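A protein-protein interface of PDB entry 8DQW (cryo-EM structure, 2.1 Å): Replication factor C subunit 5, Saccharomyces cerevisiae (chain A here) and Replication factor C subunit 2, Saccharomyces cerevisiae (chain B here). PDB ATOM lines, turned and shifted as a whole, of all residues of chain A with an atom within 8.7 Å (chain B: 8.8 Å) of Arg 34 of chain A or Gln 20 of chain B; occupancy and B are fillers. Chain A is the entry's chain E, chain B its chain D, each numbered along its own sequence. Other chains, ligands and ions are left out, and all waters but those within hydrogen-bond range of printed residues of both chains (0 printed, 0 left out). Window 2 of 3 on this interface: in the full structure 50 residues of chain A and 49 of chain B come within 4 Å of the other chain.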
ATOM      1  N   LEU A  29       1.762  18.447  36.407  1.00  0.00           N
ATOM      2  CA  LEU A  29       1.088  18.944  35.211  1.00  0.00           C
ATOM      3  C   LEU A  29       2.097  19.360  34.147  1.00  0.00           C
ATOM      4  O   LEU A  29       1.889  19.111  32.954  1.00  0.00           O
ATOM      5  CB  LEU A  29       0.177  20.119  35.569  1.00  0.00           C
ATOM      6  CG  LEU A  29      -1.215  19.776  36.108  1.00  0.00           C
ATOM      7  CD1 LEU A  29      -1.958  21.045  36.496  1.00  0.00           C
ATOM      8  CD2 LEU A  29      -2.019  18.972  35.095  1.00  0.00           C
ATOM      9  N   SER A  30       3.197  19.992  34.559  1.00  0.00           N
ATOM     10  CA  SER A  30       4.205  20.471  33.620  1.00  0.00           C
ATOM     11  C   SER A  30       5.087  19.363  33.059  1.00  0.00           C
ATOM     12  O   SER A  30       5.891  19.636  32.163  1.00  0.00           O
ATOM     13  CB  SER A  30       5.099  21.518  34.289  1.00  0.00           C
ATOM     14  OG  SER A  30       4.333  22.551  34.874  1.00  0.00           O
ATOM     15  N   ASP A  31       4.976  18.134  33.567  1.00  0.00           N
ATOM     16  CA  ASP A  31       5.839  17.060  33.086  1.00  0.00           C
ATOM     17  C   ASP A  31       5.634  16.815  31.596  1.00  0.00           C
ATOM     18  O   ASP A  31       6.598  16.779  30.821  1.00  0.00           O
ATOM     19  CB  ASP A  31       5.572  15.782  33.883  1.00  0.00           C
ATOM     20  CG  ASP A  31       6.588  14.694  33.595  1.00  0.00           C
ATOM     21  OD1 ASP A  31       7.780  15.024  33.422  1.00  0.00           O
ATOM     22  OD2 ASP A  31       6.194  13.510  33.541  1.00  0.00           O
ATOM     23  N   GLN A  32       4.381  16.651  31.174  1.00  0.00           N
ATOM     24  CA  GLN A  32       4.027  16.424  29.772  1.00  0.00           C
ATOM     25  C   GLN A  32       2.933  17.413  29.397  1.00  0.00           C
ATOM     26  O   GLN A  32       1.749  17.055  29.337  1.00  0.00           O
ATOM     27  CB  GLN A  32       3.575  14.982  29.537  1.00  0.00           C
ATOM     28  CG  GLN A  32       4.596  13.929  29.943  1.00  0.00           C
ATOM     29  CD  GLN A  32       5.664  13.716  28.887  1.00  0.00           C
ATOM     30  OE1 GLN A  32       6.765  14.257  28.985  1.00  0.00           O
ATOM     31  NE2 GLN A  32       5.341  12.927  27.870  1.00  0.00           N
ATOM     32  N   PRO A  33       3.293  18.674  29.129  1.00  0.00           N
ATOM     33  CA  PRO A  33       2.272  19.692  28.841  1.00  0.00           C
ATOM     34  C   PRO A  33       1.639  19.540  27.466  1.00  0.00           C
ATOM     35  O   PRO A  33       0.835  20.376  27.046  1.00  0.00           O
ATOM     36  CB  PRO A  33       3.071  20.994  28.952  1.00  0.00           C
ATOM     37  CG  PRO A  33       4.415  20.588  28.441  1.00  0.00           C
ATOM     38  CD  PRO A  33       4.641  19.267  29.131  1.00  0.00           C
ATOM     39  N   ARG A  34       2.004  18.469  26.761  1.00  0.00           N
ATOM     40  CA  ARG A  34       1.496  18.252  25.412  1.00  0.00           C
ATOM     41  C   ARG A  34      -0.022  18.092  25.412  1.00  0.00           C
ATOM     42  O   ARG A  34      -0.709  18.613  24.525  1.00  0.00           O
ATOM     43  CB  ARG A  34       2.196  17.030  24.809  1.00  0.00           C
ATOM     44  CG  ARG A  34       3.482  17.387  24.063  1.00  0.00           C
ATOM     45  CD  ARG A  34       3.758  16.478  22.865  1.00  0.00           C
ATOM     46  NE  ARG A  34       4.807  16.996  21.992  1.00  0.00           N
ATOM     47  CZ  ARG A  34       6.036  17.326  22.373  1.00  0.00           C
ATOM     48  NH1 ARG A  34       6.467  17.117  23.607  1.00  0.00           N
ATOM     49  NH2 ARG A  34       6.864  17.870  21.483  1.00  0.00           N
ATOM     50  N   ASP A  35      -0.565  17.393  26.407  1.00  0.00           N
ATOM     51  CA  ASP A  35      -2.000  17.146  26.521  1.00  0.00           C
ATOM     52  C   ASP A  35      -2.593  17.837  27.747  1.00  0.00           C
ATOM     53  O   ASP A  35      -3.461  17.289  28.431  1.00  0.00           O
ATOM     54  CB  ASP A  35      -2.284  15.647  26.566  1.00  0.00           C
ATOM     55  CG  ASP A  35      -1.468  14.929  27.624  1.00  0.00           C
ATOM     56  OD1 ASP A  35      -0.841  15.612  28.460  1.00  0.00           O
ATOM     57  OD2 ASP A  35      -1.452  13.681  27.615  1.00  0.00           O
ATOM     58  N   LEU A  36      -2.138  19.050  28.032  1.00  0.00           N
ATOM     59  CA  LEU A  36      -2.636  19.808  29.172  1.00  0.00           C
ATOM     60  C   LEU A  36      -4.104  20.177  28.963  1.00  0.00           C
ATOM     61  O   LEU A  36      -4.431  20.810  27.948  1.00  0.00           O
ATOM     62  CB  LEU A  36      -1.797  21.071  29.359  1.00  0.00           C
ATOM     63  CG  LEU A  36      -2.217  22.049  30.459  1.00  0.00           C
ATOM     64  CD1 LEU A  36      -1.672  21.608  31.806  1.00  0.00           C
ATOM     65  CD2 LEU A  36      -1.741  23.454  30.120  1.00  0.00           C
ATOM     66  N   PRO A  37      -5.008  19.816  29.870  1.00  0.00           N
ATOM     67  CA  PRO A  37      -6.401  20.254  29.743  1.00  0.00           C
ATOM     68  C   PRO A  37      -6.571  21.705  30.181  1.00  0.00           C
ATOM     69  O   PRO A  37      -5.680  22.322  30.763  1.00  0.00           O
ATOM     70  CB  PRO A  37      -7.171  19.308  30.676  1.00  0.00           C
ATOM     71  CG  PRO A  37      -6.204  18.226  31.052  1.00  0.00           C
ATOM     72  CD  PRO A  37      -4.850  18.840  30.961  1.00  0.00           C
ATOM     73  N   ILE A  60       6.438  25.560  31.371  1.00  0.00           N
ATOM     74  CA  ILE A  60       6.144  25.033  30.041  1.00  0.00           C
ATOM     75  C   ILE A  60       7.016  25.708  28.988  1.00  0.00           C
ATOM     76  O   ILE A  60       7.652  25.038  28.167  1.00  0.00           O
ATOM     77  CB  ILE A  60       4.648  25.196  29.716  1.00  0.00           C
ATOM     78  CG1 ILE A  60       3.810  24.253  30.580  1.00  0.00           C
ATOM     79  CG2 ILE A  60       4.392  24.919  28.240  1.00  0.00           C
ATOM     80  CD1 ILE A  60       2.460  24.816  30.957  1.00  0.00           C
ATOM     81  N   LYS A 128      14.464  21.160  11.833  1.00  0.00           N
ATOM     82  CA  LYS A 128      13.752  20.047  11.228  1.00  0.00           C
ATOM     83  C   LYS A 128      13.058  20.500   9.945  1.00  0.00           C
ATOM     84  O   LYS A 128      13.191  21.643   9.502  1.00  0.00           O
ATOM     85  CB  LYS A 128      12.758  19.458  12.228  1.00  0.00           C
ATOM     86  CG  LYS A 128      13.413  18.618  13.313  1.00  0.00           C
ATOM     87  CD  LYS A 128      12.388  17.822  14.102  1.00  0.00           C
ATOM     88  CE  LYS A 128      12.974  17.311  15.409  1.00  0.00           C
ATOM     89  NZ  LYS A 128      11.929  16.762  16.316  1.00  0.00           N
ATOM     90  N   HIS A 133       3.747  23.290  15.104  1.00  0.00           N
ATOM     91  CA  HIS A 133       2.521  23.822  15.679  1.00  0.00           C
ATOM     92  C   HIS A 133       2.640  23.878  17.196  1.00  0.00           C
ATOM     93  O   HIS A 133       3.264  23.009  17.812  1.00  0.00           O
ATOM     94  CB  HIS A 133       1.318  22.963  15.280  1.00  0.00           C
ATOM     95  CG  HIS A 133       0.045  23.349  15.967  1.00  0.00           C
ATOM     96  ND1 HIS A 133      -0.543  22.568  16.937  1.00  0.00           N
ATOM     97  CD2 HIS A 133      -0.747  24.437  15.826  1.00  0.00           C
ATOM     98  CE1 HIS A 133      -1.649  23.156  17.361  1.00  0.00           C
ATOM     99  NE2 HIS A 133      -1.794  24.292  16.704  1.00  0.00           N
ATOM    100  N   ARG A 134       2.040  24.907  17.790  1.00  0.00           N
ATOM    101  CA  ARG A 134       2.058  25.100  19.235  1.00  0.00           C
ATOM    102  C   ARG A 134       0.743  25.734  19.659  1.00  0.00           C
ATOM    103  O   ARG A 134       0.312  26.723  19.059  1.00  0.00           O
ATOM    104  CB  ARG A 134       3.232  25.991  19.655  1.00  0.00           C
ATOM    105  CG  ARG A 134       4.514  25.232  19.964  1.00  0.00           C
ATOM    106  CD  ARG A 134       5.669  26.169  20.305  1.00  0.00           C
ATOM    107  NE  ARG A 134       5.417  27.546  19.892  1.00  0.00           N
ATOM    108  CZ  ARG A 134       5.889  28.108  18.786  1.00  0.00           C
ATOM    109  NH1 ARG A 134       6.647  27.436  17.933  1.00  0.00           N
ATOM    110  NH2 ARG A 134       5.588  29.376  18.523  1.00  0.00           N
ATOM    111  N   TYR A 135       0.110  25.173  20.685  1.00  0.00           N
ATOM    112  CA  TYR A 135      -1.139  25.744  21.166  1.00  0.00           C
ATOM    113  C   TYR A 135      -0.873  27.040  21.924  1.00  0.00           C
ATOM    114  O   TYR A 135       0.180  27.224  22.540  1.00  0.00           O
ATOM    115  CB  TYR A 135      -1.897  24.744  22.047  1.00  0.00           C
ATOM    116  CG  TYR A 135      -1.236  24.362  23.361  1.00  0.00           C
ATOM    117  CD1 TYR A 135      -1.098  25.281  24.396  1.00  0.00           C
ATOM    118  CD2 TYR A 135      -0.779  23.067  23.575  1.00  0.00           C
ATOM    119  CE1 TYR A 135      -0.506  24.928  25.594  1.00  0.00           C
ATOM    120  CE2 TYR A 135      -0.188  22.705  24.771  1.00  0.00           C
ATOM    121  CZ  TYR A 135      -0.055  23.639  25.777  1.00  0.00           C
ATOM    122  OH  TYR A 135       0.532  23.282  26.968  1.00  0.00           O
ATOM    123  N   SER A 162      -9.611  22.838  20.633  1.00  0.00           N
ATOM    124  CA  SER A 162      -8.723  22.438  21.718  1.00  0.00           C
ATOM    125  C   SER A 162      -7.283  22.277  21.248  1.00  0.00           C
ATOM    126  O   SER A 162      -6.364  22.358  22.069  1.00  0.00           O
ATOM    127  CB  SER A 162      -9.210  21.130  22.346  1.00  0.00           C
ATOM    128  OG  SER A 162      -9.574  20.191  21.349  1.00  0.00           O
ATOM    129  N   LYS A 163      -7.072  22.052  19.949  1.00  0.00           N
ATOM    130  CA  LYS A 163      -5.717  21.900  19.432  1.00  0.00           C
ATOM    131  C   LYS A 163      -4.946  23.214  19.471  1.00  0.00           C
ATOM    132  O   LYS A 163      -3.727  23.209  19.675  1.00  0.00           O
ATOM    133  CB  LYS A 163      -5.760  21.365  18.000  1.00  0.00           C
ATOM    134  CG  LYS A 163      -5.539  19.866  17.881  1.00  0.00           C
ATOM    135  CD  LYS A 163      -5.893  19.363  16.485  1.00  0.00           C
ATOM    136  CE  LYS A 163      -6.536  17.989  16.533  1.00  0.00           C
ATOM    137  NZ  LYS A 163      -5.659  16.988  17.197  1.00  0.00           N
ATOM    138  N   ARG A 166      -5.560  26.666  24.942  1.00  0.00           N
ATOM    139  CA  ARG A 166      -5.780  26.076  26.258  1.00  0.00           C
ATOM    140  C   ARG A 166      -6.054  27.207  27.236  1.00  0.00           C
ATOM    141  O   ARG A 166      -5.215  28.096  27.408  1.00  0.00           O
ATOM    142  CB  ARG A 166      -4.574  25.247  26.713  1.00  0.00           C
ATOM    143  CG  ARG A 166      -4.168  24.143  25.747  1.00  0.00           C
ATOM    144  CD  ARG A 166      -5.213  23.040  25.673  1.00  0.00           C
ATOM    145  NE  ARG A 166      -5.003  22.173  24.520  1.00  0.00           N
ATOM    146  CZ  ARG A 166      -4.078  21.224  24.446  1.00  0.00           C
ATOM    147  NH1 ARG A 166      -3.263  20.972  25.457  1.00  0.00           N
ATOM    148  NH2 ARG A 166      -3.968  20.512  23.329  1.00  0.00           N
ATOM    149  N   GLU B  19       3.734   9.635  17.430  1.00  0.00           N
ATOM    150  CA  GLU B  19       2.996   9.389  18.663  1.00  0.00           C
ATOM    151  C   GLU B  19       2.728  10.695  19.403  1.00  0.00           C
ATOM    152  O   GLU B  19       1.738  10.820  20.124  1.00  0.00           O
ATOM    153  CB  GLU B  19       3.767   8.424  19.564  1.00  0.00           C
ATOM    154  N   GLN B  20       3.620  11.671  19.218  1.00  0.00           N
ATOM    155  CA  GLN B  20       3.452  12.961  19.882  1.00  0.00           C
ATOM    156  C   GLN B  20       2.184  13.662  19.412  1.00  0.00           C
ATOM    157  O   GLN B  20       1.464  14.264  20.216  1.00  0.00           O
ATOM    158  CB  GLN B  20       4.676  13.841  19.629  1.00  0.00           C
ATOM    159  N   SER B  21       1.895  13.599  18.109  1.00  0.00           N
ATOM    160  CA  SER B  21       0.706  14.262  17.585  1.00  0.00           C
ATOM    161  C   SER B  21      -0.564  13.678  18.191  1.00  0.00           C
ATOM    162  O   SER B  21      -1.495  14.416  18.530  1.00  0.00           O
ATOM    163  CB  SER B  21       0.674  14.150  16.061  1.00  0.00           C
ATOM    164  OG  SER B  21      -0.280  15.038  15.505  1.00  0.00           O
ATOM    165  N   LEU B  22      -0.625  12.352  18.328  1.00  0.00           N
ATOM    166  CA  LEU B  22      -1.795  11.732  18.938  1.00  0.00           C
ATOM    167  C   LEU B  22      -1.920  12.102  20.412  1.00  0.00           C
ATOM    168  O   LEU B  22      -3.021  12.041  20.973  1.00  0.00           O
ATOM    169  CB  LEU B  22      -1.733  10.214  18.771  1.00  0.00           C
ATOM    170  CG  LEU B  22      -1.820   9.705  17.328  1.00  0.00           C
ATOM    171  CD1 LEU B  22      -1.520   8.215  17.262  1.00  0.00           C
ATOM    172  CD2 LEU B  22      -3.186  10.008  16.726  1.00  0.00           C
ATOM    173  N   ALA B  23      -0.815  12.483  21.053  1.00  0.00           N
ATOM    174  CA  ALA B  23      -0.813  12.881  22.454  1.00  0.00           C
ATOM    175  C   ALA B  23      -0.930  14.392  22.635  1.00  0.00           C
ATOM    176  O   ALA B  23      -0.536  14.914  23.684  1.00  0.00           O
ATOM    177  CB  ALA B  23       0.453  12.368  23.143  1.00  0.00           C
ATOM    178  N   GLN B  24      -1.459  15.100  21.638  1.00  0.00           N
ATOM    179  CA  GLN B  24      -1.676  16.540  21.708  1.00  0.00           C
ATOM    180  C   GLN B  24      -3.063  16.922  22.197  1.00  0.00           C
ATOM    181  O   GLN B  24      -3.372  18.115  22.257  1.00  0.00           O
ATOM    182  CB  GLN B  24      -1.447  17.173  20.330  1.00  0.00           C
ATOM    183  CG  GLN B  24      -0.124  17.894  20.131  1.00  0.00           C
ATOM    184  CD  GLN B  24       0.292  18.729  21.331  1.00  0.00           C
ATOM    185  OE1 GLN B  24      -0.256  19.805  21.576  1.00  0.00           O
ATOM    186  NE2 GLN B  24       1.253  18.232  22.085  1.00  0.00           N
ATOM    187  N   GLN B  25      -3.904  15.952  22.549  1.00  0.00           N
ATOM    188  CA  GLN B  25      -5.281  16.266  22.864  1.00  0.00           C
ATOM    189  C   GLN B  25      -5.632  15.811  24.275  1.00  0.00           C
ATOM    190  O   GLN B  25      -5.265  14.702  24.675  1.00  0.00           O
ATOM    191  CB  GLN B  25      -6.231  15.598  21.861  1.00  0.00           C
ATOM    192  CG  GLN B  25      -6.364  16.357  20.550  1.00  0.00           C
ATOM    193  CD  GLN B  25      -7.391  17.471  20.621  1.00  0.00           C
ATOM    194  OE1 GLN B  25      -7.239  18.420  21.390  1.00  0.00           O
ATOM    195  NE2 GLN B  25      -8.438  17.364  19.812  1.00  0.00           N
ATOM    196  N   PRO B  26      -6.322  16.643  25.055  1.00  0.00           N
ATOM    197  CA  PRO B  26      -6.886  16.157  26.317  1.00  0.00           C
ATOM    198  C   PRO B  26      -7.731  14.915  26.087  1.00  0.00           C
ATOM    199  O   PRO B  26      -8.243  14.676  24.991  1.00  0.00           O
ATOM    200  CB  PRO B  26      -7.732  17.337  26.802  1.00  0.00           C
ATOM    201  CG  PRO B  26      -7.029  18.529  26.252  1.00  0.00           C
ATOM    202  CD  PRO B  26      -6.489  18.100  24.910  1.00  0.00           C
ATOM    203  N   LYS B  30      -9.711  13.509  22.985  1.00  0.00           N
ATOM    204  CA  LYS B  30      -9.081  12.343  22.376  1.00  0.00           C
ATOM    205  C   LYS B  30     -10.069  11.192  22.238  1.00  0.00           C
ATOM    206  O   LYS B  30     -10.116  10.528  21.196  1.00  0.00           O
ATOM    207  CB  LYS B  30      -7.874  11.911  23.208  1.00  0.00           C
ATOM    208  CG  LYS B  30      -7.126  10.704  22.652  1.00  0.00           C
ATOM    209  CD  LYS B  30      -6.128  10.157  23.660  1.00  0.00           C
ATOM    210  CE  LYS B  30      -4.697  10.364  23.201  1.00  0.00           C
ATOM    211  NZ  LYS B  30      -4.268   9.287  22.267  1.00  0.00           N
ATOM    212  N   GLN B 236      -7.544  11.559  33.954  1.00  0.00           N
ATOM    213  CA  GLN B 236      -6.322  12.087  33.356  1.00  0.00           C
ATOM    214  C   GLN B 236      -5.440  12.758  34.401  1.00  0.00           C
ATOM    215  O   GLN B 236      -4.215  12.588  34.391  1.00  0.00           O
ATOM    216  CB  GLN B 236      -6.657  13.076  32.242  1.00  0.00           C
ATOM    217  CG  GLN B 236      -5.471  13.384  31.335  1.00  0.00           C
ATOM    218  CD  GLN B 236      -5.757  14.470  30.308  1.00  0.00           C
ATOM    219  OE1 GLN B 236      -4.835  15.006  29.693  1.00  0.00           O
ATOM    220  NE2 GLN B 236      -7.029  14.806  30.121  1.00  0.00           N
ATOM    221  N   LYS B 240      -1.674  11.626  35.382  1.00  0.00           N
ATOM    222  CA  LYS B 240      -0.532  12.531  35.331  1.00  0.00           C
ATOM    223  C   LYS B 240       0.210  12.549  36.660  1.00  0.00           C
ATOM    224  O   LYS B 240       1.447  12.504  36.693  1.00  0.00           O
ATOM    225  CB  LYS B 240      -0.990  13.941  34.961  1.00  0.00           C
ATOM    226  CG  LYS B 240      -1.240  14.145  33.478  1.00  0.00           C
ATOM    227  CD  LYS B 240      -1.355  15.621  33.134  1.00  0.00           C
ATOM    228  CE  LYS B 240      -1.470  15.831  31.633  1.00  0.00           C
ATOM    229  NZ  LYS B 240      -0.148  15.736  30.956  1.00  0.00           N
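NE2 of Gln 24 of chain B sits close to O of Arg 34 of chain A, 3.2 Å away.
The backbone carbonyl oxygen (O) of Gln 24 of chain B is in hydrogen-bond range of the guanidinium group (NH2) of Arg 166 of chain A, 2.7 Å away.
The side-chain hydroxyl of Ser 162 of chain A is in hydrogen-bond range of the side-chain amide oxygen of Gln 25 of chain B (2.9 Å).
OE1 of Gln 236 of chain B lies close to O of Asp 35 of chain A, 2.9 Å away.
The side-chain amino group (NZ) of Lys 240 of chain B is in hydrogen-bond range of the backbone carbonyl oxygen (O) of Gln 32 of chain A, at 2.8 Å.
NZ of Lys 240 of chain B is in salt-bridge range of OD1 of Asp 35 of chain A (2.6 Å).
The backbone carbonyl oxygen (O) of Pro 33 of chain A sits at hydrogen-bond distance from the side-chain hydroxyl (OH) of Tyr 135 of chain A, 2.9 Å away.
The backbone carbonyl oxygen (O) of Leu 36 of chain A lies within hydrogen-bond range of the guanidinium group (NH1) of Arg 166 of chain A (2.8 Å).
NE of Arg 166 of chain A lies within hydrogen-bond range of O of Ser 162 of chain A, 2.8 Å away.
Leu 29 of chain A touches Lys 240 of chain B.
Arg 34 of chain A touches Gln 20 of chain B (NE to CB, 3.9 Å).
O of Ala 23 of chain B touches CB of Arg 34 of chain A (3.6 Å).
O of Gln 25 of chain B touches CB of Asp 35 of chain A (3.7 Å).
O of Leu 36 of chain A touches CG of Pro 26 of chain B, at 3.9 Å.
CA of Pro 37 of chain A touches CG of Pro 26 of chain B (3.9 Å).
Pro 37 of chain A touches Gln 236 of chain B (CG to NE2, 3.6 Å).
Gln 24 of chain B touches Tyr 135 of chain A.
NZ of Lys 163 of chain A touches CG of Gln 25 of chain B, 3.5 Å away.
Pro 26 of chain B touches Arg 166 of chain A.
Of chain A, only Arg 34 (3.9 Å) comes within 4 Å of Gln 20 of chain B.
No residue of chain A comes within 4 Å of Glu 19 of chain B.
Of the printed residues of chain A, Lys 240 of chain B touches Leu 29 (3.9 Å), Gln 32 (2.8 Å) and Asp 35 (2.6 Å).
Printed residues of chain B within 4 Å of Pro 37 of chain A: Pro 26 (3.9 Å) and Gln 236 (3.6 Å).
Of the printed residues of chain B, Ser 162 of chain A touches Gln 25.
Printed residues of chain B within 4 Å of Leu 29 of chain A: Lys 240.
Lys 30 of chain B touches none of the printed residues of chain A.
Ile 60 of chain A touches none of the printed residues of chain B.
The nearest residue of chain B that does not touch Arg 34 of chain A is Gln 25 of chain B (4.6 Å).
The nearest residue of chain A that does not touch Gln 20 of chain B is Asp 35 of chain A (7.2 Å).
Of the 11 printed residues of chain B, 7 touch a printed residue of chain A.
Hydrophobic or aromatic side chains of chain B that line the printed part of chain A: Pro 26.
Along chain B the printed residues that touch a printed residue of chain A span positions 20 to 240.
Among the printed residues, 17 pairs touch across the chains.
Among the printed residues, Asp or Glu carboxylates within 4 Å of a Lys or Arg side-chain nitrogen of the other chain: Asp 35 of chain A with Lys 240 of chain B (2.6 Å).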
